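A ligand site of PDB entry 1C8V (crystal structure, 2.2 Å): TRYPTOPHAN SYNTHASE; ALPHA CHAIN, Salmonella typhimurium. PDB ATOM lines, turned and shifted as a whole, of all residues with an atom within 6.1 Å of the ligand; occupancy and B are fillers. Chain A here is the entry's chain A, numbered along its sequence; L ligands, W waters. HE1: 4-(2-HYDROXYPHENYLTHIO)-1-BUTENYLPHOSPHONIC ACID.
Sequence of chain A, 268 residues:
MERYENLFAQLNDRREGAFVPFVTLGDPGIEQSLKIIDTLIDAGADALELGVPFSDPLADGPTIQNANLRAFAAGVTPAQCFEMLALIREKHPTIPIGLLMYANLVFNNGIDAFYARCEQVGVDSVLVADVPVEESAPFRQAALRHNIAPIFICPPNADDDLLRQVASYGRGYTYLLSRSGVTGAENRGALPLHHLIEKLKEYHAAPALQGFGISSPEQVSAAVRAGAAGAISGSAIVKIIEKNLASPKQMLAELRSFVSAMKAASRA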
ATOM      1  N   PHE A  22      21.322 -33.760  22.364  1.00  0.00           N
ATOM      2  CA  PHE A  22      20.826 -33.683  20.995  1.00  0.00           C
ATOM      3  C   PHE A  22      22.002 -33.688  20.004  1.00  0.00           C
ATOM      4  O   PHE A  22      23.085 -33.193  20.312  1.00  0.00           O
ATOM      5  CB  PHE A  22      19.959 -32.421  20.798  1.00  0.00           C
ATOM      6  CG  PHE A  22      19.649 -32.102  19.337  1.00  0.00           C
ATOM      7  CD1 PHE A  22      20.594 -31.442  18.531  1.00  0.00           C
ATOM      8  CD2 PHE A  22      18.422 -32.451  18.778  1.00  0.00           C
ATOM      9  CE1 PHE A  22      20.320 -31.151  17.201  1.00  0.00           C
ATOM     10  CE2 PHE A  22      18.135 -32.161  17.436  1.00  0.00           C
ATOM     11  CZ  PHE A  22      19.088 -31.513  16.648  1.00  0.00           C
ATOM     12  N   GLU A  49      17.503 -37.193  21.671  1.00  0.00           N
ATOM     13  CA  GLU A  49      16.776 -36.208  20.841  1.00  0.00           C
ATOM     14  C   GLU A  49      17.608 -36.147  19.554  1.00  0.00           C
ATOM     15  O   GLU A  49      18.779 -35.728  19.574  1.00  0.00           O
ATOM     16  CB  GLU A  49      16.734 -34.860  21.558  1.00  0.00           C
ATOM     17  CG  GLU A  49      15.563 -33.928  21.214  1.00  0.00           C
ATOM     18  CD  GLU A  49      14.185 -34.571  21.217  1.00  0.00           C
ATOM     19  OE1 GLU A  49      13.789 -35.172  22.255  1.00  0.00           O
ATOM     20  OE2 GLU A  49      13.490 -34.435  20.178  1.00  0.00           O
ATOM     21  N   ALA A  59      14.195 -22.740  13.268  1.00  0.00           N
ATOM     22  CA  ALA A  59      14.065 -22.591  14.719  1.00  0.00           C
ATOM     23  C   ALA A  59      15.414 -22.881  15.382  1.00  0.00           C
ATOM     24  O   ALA A  59      15.515 -22.931  16.619  1.00  0.00           O
ATOM     25  CB  ALA A  59      12.990 -23.523  15.259  1.00  0.00           C
ATOM     26  N   ASP A  60      16.462 -22.953  14.562  1.00  0.00           N
ATOM     27  CA  ASP A  60      17.804 -23.254  15.024  1.00  0.00           C
ATOM     28  C   ASP A  60      18.856 -22.171  14.776  1.00  0.00           C
ATOM     29  O   ASP A  60      18.909 -21.573  13.695  1.00  0.00           O
ATOM     30  CB  ASP A  60      18.293 -24.567  14.381  1.00  0.00           C
ATOM     31  CG  ASP A  60      17.587 -25.798  14.945  1.00  0.00           C
ATOM     32  OD1 ASP A  60      17.796 -26.102  16.134  1.00  0.00           O
ATOM     33  OD2 ASP A  60      16.827 -26.472  14.209  1.00  0.00           O
ATOM     34  N   ILE A  64      23.618 -25.439  15.245  1.00  0.00           N
ATOM     35  CA  ILE A  64      22.813 -26.511  14.672  1.00  0.00           C
ATOM     36  C   ILE A  64      22.607 -26.344  13.152  1.00  0.00           C
ATOM     37  O   ILE A  64      22.498 -27.339  12.414  1.00  0.00           O
ATOM     38  CB  ILE A  64      21.507 -26.695  15.476  1.00  0.00           C
ATOM     39  CG1 ILE A  64      21.858 -27.289  16.844  1.00  0.00           C
ATOM     40  CG2 ILE A  64      20.528 -27.614  14.742  1.00  0.00           C
ATOM     41  CD1 ILE A  64      20.666 -27.449  17.795  1.00  0.00           C
ATOM     42  N   LEU A 100      13.445 -34.664  16.177  1.00  0.00           N
ATOM     43  CA  LEU A 100      13.144 -33.231  16.054  1.00  0.00           C
ATOM     44  C   LEU A 100      12.940 -33.117  14.544  1.00  0.00           C
ATOM     45  O   LEU A 100      13.876 -33.344  13.760  1.00  0.00           O
ATOM     46  CB  LEU A 100      14.302 -32.331  16.519  1.00  0.00           C
ATOM     47  CG  LEU A 100      14.056 -30.805  16.450  1.00  0.00           C
ATOM     48  CD1 LEU A 100      14.181 -30.259  15.046  1.00  0.00           C
ATOM     49  CD2 LEU A 100      12.697 -30.464  17.018  1.00  0.00           C
ATOM     50  N   TYR A 102      10.893 -30.988  11.044  1.00  0.00           N
ATOM     51  CA  TYR A 102      10.325 -29.767  10.477  1.00  0.00           C
ATOM     52  C   TYR A 102       9.138 -30.324   9.679  1.00  0.00           C
ATOM     53  O   TYR A 102       9.213 -31.442   9.182  1.00  0.00           O
ATOM     54  CB  TYR A 102      11.346 -29.015   9.628  1.00  0.00           C
ATOM     55  CG  TYR A 102      12.204 -28.107  10.481  1.00  0.00           C
ATOM     56  CD1 TYR A 102      11.740 -26.851  10.883  1.00  0.00           C
ATOM     57  CD2 TYR A 102      13.442 -28.539  10.968  1.00  0.00           C
ATOM     58  CE1 TYR A 102      12.471 -26.049  11.760  1.00  0.00           C
ATOM     59  CE2 TYR A 102      14.195 -27.736  11.846  1.00  0.00           C
ATOM     60  CZ  TYR A 102      13.692 -26.494  12.240  1.00  0.00           C
ATOM     61  OH  TYR A 102      14.405 -25.710  13.119  1.00  0.00           O
ATOM     62  N   LEU A 127       8.577 -34.368  17.817  1.00  0.00           N
ATOM     63  CA  LEU A 127       8.335 -32.947  18.052  1.00  0.00           C
ATOM     64  C   LEU A 127       8.536 -32.278  16.694  1.00  0.00           C
ATOM     65  O   LEU A 127       9.607 -32.411  16.090  1.00  0.00           O
ATOM     66  CB  LEU A 127       9.353 -32.381  19.051  1.00  0.00           C
ATOM     67  CG  LEU A 127       9.483 -30.850  19.116  1.00  0.00           C
ATOM     68  CD1 LEU A 127       8.137 -30.198  19.458  1.00  0.00           C
ATOM     69  CD2 LEU A 127      10.534 -30.450  20.133  1.00  0.00           C
ATOM     70  N   ALA A 129       8.913 -28.920  15.007  1.00  0.00           N
ATOM     71  CA  ALA A 129       9.236 -27.531  15.370  1.00  0.00           C
ATOM     72  C   ALA A 129       8.308 -26.413  14.869  1.00  0.00           C
ATOM     73  O   ALA A 129       8.065 -25.428  15.593  1.00  0.00           O
ATOM     74  CB  ALA A 129      10.707 -27.209  15.038  1.00  0.00           C
ATOM     75  N   ILE A 153       5.169 -27.937  22.738  1.00  0.00           N
ATOM     76  CA  ILE A 153       6.032 -26.918  23.345  1.00  0.00           C
ATOM     77  C   ILE A 153       5.231 -25.929  24.201  1.00  0.00           C
ATOM     78  O   ILE A 153       4.240 -25.351  23.748  1.00  0.00           O
ATOM     79  CB  ILE A 153       6.880 -26.132  22.282  1.00  0.00           C
ATOM     80  CG1 ILE A 153       8.010 -27.029  21.778  1.00  0.00           C
ATOM     81  CG2 ILE A 153       7.441 -24.812  22.870  1.00  0.00           C
ATOM     82  CD1 ILE A 153       9.065 -26.312  20.971  1.00  0.00           C
ATOM     83  N   TYR A 175       7.835 -30.324  26.392  1.00  0.00           N
ATOM     84  CA  TYR A 175       9.035 -29.537  26.124  1.00  0.00           C
ATOM     85  C   TYR A 175       8.866 -28.140  26.702  1.00  0.00           C
ATOM     86  O   TYR A 175       8.144 -27.325  26.137  1.00  0.00           O
ATOM     87  CB  TYR A 175       9.311 -29.445  24.622  1.00  0.00           C
ATOM     88  CG  TYR A 175      10.743 -29.072  24.244  1.00  0.00           C
ATOM     89  CD1 TYR A 175      11.270 -27.807  24.544  1.00  0.00           C
ATOM     90  CD2 TYR A 175      11.568 -29.980  23.576  1.00  0.00           C
ATOM     91  CE1 TYR A 175      12.576 -27.456  24.183  1.00  0.00           C
ATOM     92  CE2 TYR A 175      12.869 -29.641  23.220  1.00  0.00           C
ATOM     93  CZ  TYR A 175      13.369 -28.385  23.515  1.00  0.00           C
ATOM     94  OH  TYR A 175      14.655 -28.051  23.134  1.00  0.00           O
ATOM     95  N   LEU A 177      10.216 -24.647  27.243  1.00  0.00           N
ATOM     96  CA  LEU A 177      11.179 -23.700  26.703  1.00  0.00           C
ATOM     97  C   LEU A 177      11.768 -22.802  27.797  1.00  0.00           C
ATOM     98  O   LEU A 177      11.034 -22.183  28.564  1.00  0.00           O
ATOM     99  CB  LEU A 177      10.484 -22.836  25.637  1.00  0.00           C
ATOM    100  CG  LEU A 177      10.966 -22.812  24.183  1.00  0.00           C
ATOM    101  CD1 LEU A 177      11.375 -24.179  23.687  1.00  0.00           C
ATOM    102  CD2 LEU A 177       9.845 -22.231  23.332  1.00  0.00           C
ATOM    103  N   ARG A 179      13.682 -20.201  27.139  1.00  0.00           N
ATOM    104  CA  ARG A 179      13.794 -18.875  26.548  1.00  0.00           C
ATOM    105  C   ARG A 179      12.902 -18.611  25.323  1.00  0.00           C
ATOM    106  O   ARG A 179      12.278 -19.505  24.751  1.00  0.00           O
ATOM    107  CB  ARG A 179      15.230 -18.817  25.992  1.00  0.00           C
ATOM    108  CG  ARG A 179      16.099 -17.704  26.411  1.00  0.00           C
ATOM    109  CD  ARG A 179      17.243 -17.539  25.394  1.00  0.00           C
ATOM    110  NE  ARG A 179      18.007 -18.752  25.093  1.00  0.00           N
ATOM    111  CZ  ARG A 179      17.966 -19.401  23.919  1.00  0.00           C
ATOM    112  NH1 ARG A 179      17.171 -18.994  22.936  1.00  0.00           N
ATOM    113  NH2 ARG A 179      18.801 -20.406  23.689  1.00  0.00           N
ATOM    114  N   VAL A 182      15.746 -18.764  19.290  1.00  0.00           N
ATOM    115  CA  VAL A 182      16.103 -20.033  18.658  1.00  0.00           C
ATOM    116  C   VAL A 182      17.172 -20.780  19.457  1.00  0.00           C
ATOM    117  O   VAL A 182      17.723 -20.229  20.412  1.00  0.00           O
ATOM    118  CB  VAL A 182      16.632 -19.839  17.203  1.00  0.00           C
ATOM    119  CG1 VAL A 182      15.608 -19.120  16.340  1.00  0.00           C
ATOM    120  CG2 VAL A 182      17.956 -19.092  17.209  1.00  0.00           C
ATOM    121  N   THR A 183      17.483 -22.010  19.047  1.00  0.00           N
ATOM    122  CA  THR A 183      18.479 -22.828  19.735  1.00  0.00           C
ATOM    123  C   THR A 183      19.841 -22.148  19.746  1.00  0.00           C
ATOM    124  O   THR A 183      20.159 -21.356  18.862  1.00  0.00           O
ATOM    125  CB  THR A 183      18.630 -24.252  19.101  1.00  0.00           C
ATOM    126  OG1 THR A 183      19.295 -24.176  17.821  1.00  0.00           O
ATOM    127  CG2 THR A 183      17.279 -24.909  18.925  1.00  0.00           C
ATOM    128  N   GLY A 184      20.638 -22.453  20.763  1.00  0.00           N
ATOM    129  CA  GLY A 184      21.968 -21.875  20.848  1.00  0.00           C
ATOM    130  C   GLY A 184      22.484 -21.861  22.257  1.00  0.00           C
ATOM    131  O   GLY A 184      21.815 -21.331  23.154  1.00  0.00           O
ATOM    132  N   ALA A 185      23.633 -22.493  22.489  1.00  0.00           N
ATOM    133  CA  ALA A 185      24.238 -22.534  23.826  1.00  0.00           C
ATOM    134  C   ALA A 185      24.854 -21.155  24.126  1.00  0.00           C
ATOM    135  O   ALA A 185      25.235 -20.861  25.266  1.00  0.00           O
ATOM    136  CB  ALA A 185      25.315 -23.614  23.883  1.00  0.00           C
ATOM    137  N   GLY A 211      14.388 -27.146  27.691  1.00  0.00           N
ATOM    138  CA  GLY A 211      15.282 -27.026  26.552  1.00  0.00           C
ATOM    139  C   GLY A 211      15.566 -25.588  26.117  1.00  0.00           C
ATOM    140  O   GLY A 211      14.722 -24.724  26.297  1.00  0.00           O
ATOM    141  N   PHE A 212      16.755 -25.381  25.535  1.00  0.00           N
ATOM    142  CA  PHE A 212      17.271 -24.099  25.025  1.00  0.00           C
ATOM    143  C   PHE A 212      18.238 -23.409  25.987  1.00  0.00           C
ATOM    144  O   PHE A 212      17.850 -22.991  27.081  1.00  0.00           O
ATOM    145  CB  PHE A 212      16.146 -23.101  24.646  1.00  0.00           C
ATOM    146  CG  PHE A 212      15.474 -23.386  23.308  1.00  0.00           C
ATOM    147  CD1 PHE A 212      15.000 -22.328  22.535  1.00  0.00           C
ATOM    148  CD2 PHE A 212      15.274 -24.685  22.859  1.00  0.00           C
ATOM    149  CE1 PHE A 212      14.329 -22.566  21.326  1.00  0.00           C
ATOM    150  CE2 PHE A 212      14.608 -24.939  21.654  1.00  0.00           C
ATOM    151  CZ  PHE A 212      14.134 -23.881  20.881  1.00  0.00           C
ATOM    152  N   GLY A 213      19.513 -23.305  25.572  1.00  0.00           N
ATOM    153  CA  GLY A 213      20.548 -22.636  26.355  1.00  0.00           C
ATOM    154  C   GLY A 213      21.269 -23.416  27.447  1.00  0.00           C
ATOM    155  O   GLY A 213      22.177 -22.890  28.096  1.00  0.00           O
ATOM    156  N   ILE A 214      20.882 -24.674  27.670  1.00  0.00           N
ATOM    157  CA  ILE A 214      21.494 -25.517  28.695  1.00  0.00           C
ATOM    158  C   ILE A 214      22.865 -25.991  28.224  1.00  0.00           C
ATOM    159  O   ILE A 214      22.960 -26.765  27.265  1.00  0.00           O
ATOM    160  CB  ILE A 214      20.617 -26.768  28.979  1.00  0.00           C
ATOM    161  CG1 ILE A 214      19.151 -26.381  29.212  1.00  0.00           C
ATOM    162  CG2 ILE A 214      21.175 -27.545  30.150  1.00  0.00           C
ATOM    163  CD1 ILE A 214      18.904 -25.704  30.512  1.00  0.00           C
ATOM    164  N   SER A 215      23.931 -25.527  28.877  1.00  0.00           N
ATOM    165  CA  SER A 215      25.273 -25.960  28.476  1.00  0.00           C
ATOM    166  C   SER A 215      26.230 -26.284  29.635  1.00  0.00           C
ATOM    167  O   SER A 215      27.333 -26.788  29.396  1.00  0.00           O
ATOM    168  CB  SER A 215      25.898 -24.927  27.539  1.00  0.00           C
ATOM    169  OG  SER A 215      25.912 -23.652  28.151  1.00  0.00           O
ATOM    170  N   ILE A 232      17.444 -30.919  28.322  1.00  0.00           N
ATOM    171  CA  ILE A 232      17.932 -31.232  26.975  1.00  0.00           C
ATOM    172  C   ILE A 232      19.075 -30.245  26.636  1.00  0.00           C
ATOM    173  O   ILE A 232      18.977 -29.050  26.936  1.00  0.00           O
ATOM    174  CB  ILE A 232      16.784 -31.061  25.924  1.00  0.00           C
ATOM    175  CG1 ILE A 232      15.641 -32.011  26.234  1.00  0.00           C
ATOM    176  CG2 ILE A 232      17.303 -31.329  24.500  1.00  0.00           C
ATOM    177  CD1 ILE A 232      14.378 -31.717  25.448  1.00  0.00           C
ATOM    178  N   SER A 233      20.135 -30.750  26.024  1.00  0.00           N
ATOM    179  CA  SER A 233      21.287 -29.919  25.653  1.00  0.00           C
ATOM    180  C   SER A 233      21.715 -30.280  24.237  1.00  0.00           C
ATOM    181  O   SER A 233      21.999 -31.451  23.959  1.00  0.00           O
ATOM    182  CB  SER A 233      22.446 -30.152  26.645  1.00  0.00           C
ATOM    183  OG  SER A 233      23.603 -29.401  26.315  1.00  0.00           O
ATOM    184  N   GLY A 234      21.773 -29.293  23.345  1.00  0.00           N
ATOM    185  CA  GLY A 234      22.159 -29.550  21.950  1.00  0.00           C
ATOM    186  C   GLY A 234      23.410 -28.860  21.426  1.00  0.00           C
ATOM    187  O   GLY A 234      24.407 -29.525  21.123  1.00  0.00           O
ATOM    188  N   SER A 235      23.387 -27.534  21.361  1.00  0.00           N
ATOM    189  CA  SER A 235      24.539 -26.775  20.860  1.00  0.00           C
ATOM    190  C   SER A 235      25.861 -27.064  21.576  1.00  0.00           C
ATOM    191  O   SER A 235      26.935 -27.018  20.940  1.00  0.00           O
ATOM    192  CB  SER A 235      24.238 -25.279  20.884  1.00  0.00           C
ATOM    193  OG  SER A 235      23.139 -24.966  20.050  1.00  0.00           O
ATOM    194  N   ALA A 236      25.808 -27.324  22.878  1.00  0.00           N
ATOM    195  CA  ALA A 236      27.012 -27.621  23.627  1.00  0.00           C
ATOM    196  C   ALA A 236      27.585 -28.972  23.191  1.00  0.00           C
ATOM    197  O   ALA A 236      28.811 -29.153  23.163  1.00  0.00           O
ATOM    198  CB  ALA A 236      26.734 -27.612  25.140  1.00  0.00           C
HETATM  199  P1  HE1 L   1      20.131 -25.826  22.589  1.00  0.00           P
HETATM  200  O1  HE1 L   1      21.172 -25.941  21.478  1.00  0.00           O
HETATM  201  O2  HE1 L   1      20.145 -24.376  22.971  1.00  0.00           O
HETATM  202  O3  HE1 L   1      20.796 -26.533  23.785  1.00  0.00           O
HETATM  203  C1  HE1 L   1      18.582 -26.415  22.148  1.00  0.00           C
HETATM  204  C2  HE1 L   1      18.594 -27.804  21.499  1.00  0.00           C
HETATM  205  C3  HE1 L   1      17.165 -29.466  20.234  1.00  0.00           C
HETATM  206  C4  HE1 L   1      17.185 -28.262  21.154  1.00  0.00           C
HETATM  207  S1  HE1 L   1      15.433 -29.872  19.916  1.00  0.00           S
HETATM  208  OH  HE1 L   1      16.274 -27.971  17.510  1.00  0.00           O
HETATM  209  C5  HE1 L   1      13.115 -26.296  18.294  1.00  0.00           C
HETATM  210  C6  HE1 L   1      14.333 -26.627  17.690  1.00  0.00           C
HETATM  211  C7  HE1 L   1      15.088 -27.704  18.144  1.00  0.00           C
HETATM  212  C8  HE1 L   1      14.587 -28.475  19.244  1.00  0.00           C
HETATM  213  C9  HE1 L   1      13.366 -28.149  19.836  1.00  0.00           C
HETATM  214  C10 HE1 L   1      12.625 -27.059  19.366  1.00  0.00           C
HETATM  215  O   HOH W   1      19.313 -26.547  25.936  1.00  0.00           O
HETATM  216  O   HOH W   2      23.285 -26.786  24.606  1.00  0.00           O
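The backbone NH (N) of Ser 235 sits at hydrogen-bond distance from an oxygen (O1) of the ligand (2.7 Å).
O1 of the ligand lies within hydrogen-bond range of OG of Ser 235 (2.6 Å).
The side-chain carboxylate (OD1) of Asp 60 sits at hydrogen-bond distance from an oxygen (OH) of the ligand, at 2.8 Å.
The backbone NH (N) of Gly 213 sits at hydrogen-bond distance from an oxygen (O2) of the ligand (2.9 Å).
N of Gly 234 is in hydrogen-bond range of O3 of the ligand, 3.0 Å away.
N of Gly 184 is in hydrogen-bond range of O2 of the ligand.
S1 of the ligand lies close to OH of Tyr 175, 3.8 Å away.
The side-chain carboxylate of Asp 60 sits at hydrogen-bond distance from the side-chain hydroxyl of Thr 183 (3.0 Å).
The side-chain hydroxyl of Tyr 102 is in hydrogen-bond range of the side-chain carboxylate of Asp 60 (2.8 Å).
The guanidinium group of Arg 179 is in hydrogen-bond range of the backbone carbonyl oxygen of Gly 184 (3.2 Å).
The backbone carbonyl oxygen (O) of Ala 59 is in hydrogen-bond range of the backbone NH (N) of Thr 183, 3.3 Å away.
The backbone NH of Phe 22 sits at hydrogen-bond distance from the backbone carbonyl oxygen of Ser 233 (2.9 Å).
The side-chain hydroxyl of Ser 233 is in hydrogen-bond range of the backbone carbonyl oxygen of Ile 214, at 2.9 Å.
Merely in contact with the ligand: Thr 183, Leu 100, Phe 212, Phe 22, Leu 127, Ser 233, Ile 153 and Ala 185.
Hydrophobic or aromatic side chains within 4 Å of the ligand: Phe 22, Leu 100, Leu 127, Ile 153, Tyr 175 and Phe 212.
Of the 27 residues printed, 14 come within 4 Å of the ligand.
The nearest printed residue that does not touch the ligand is Ile 64 (4.01 Å).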
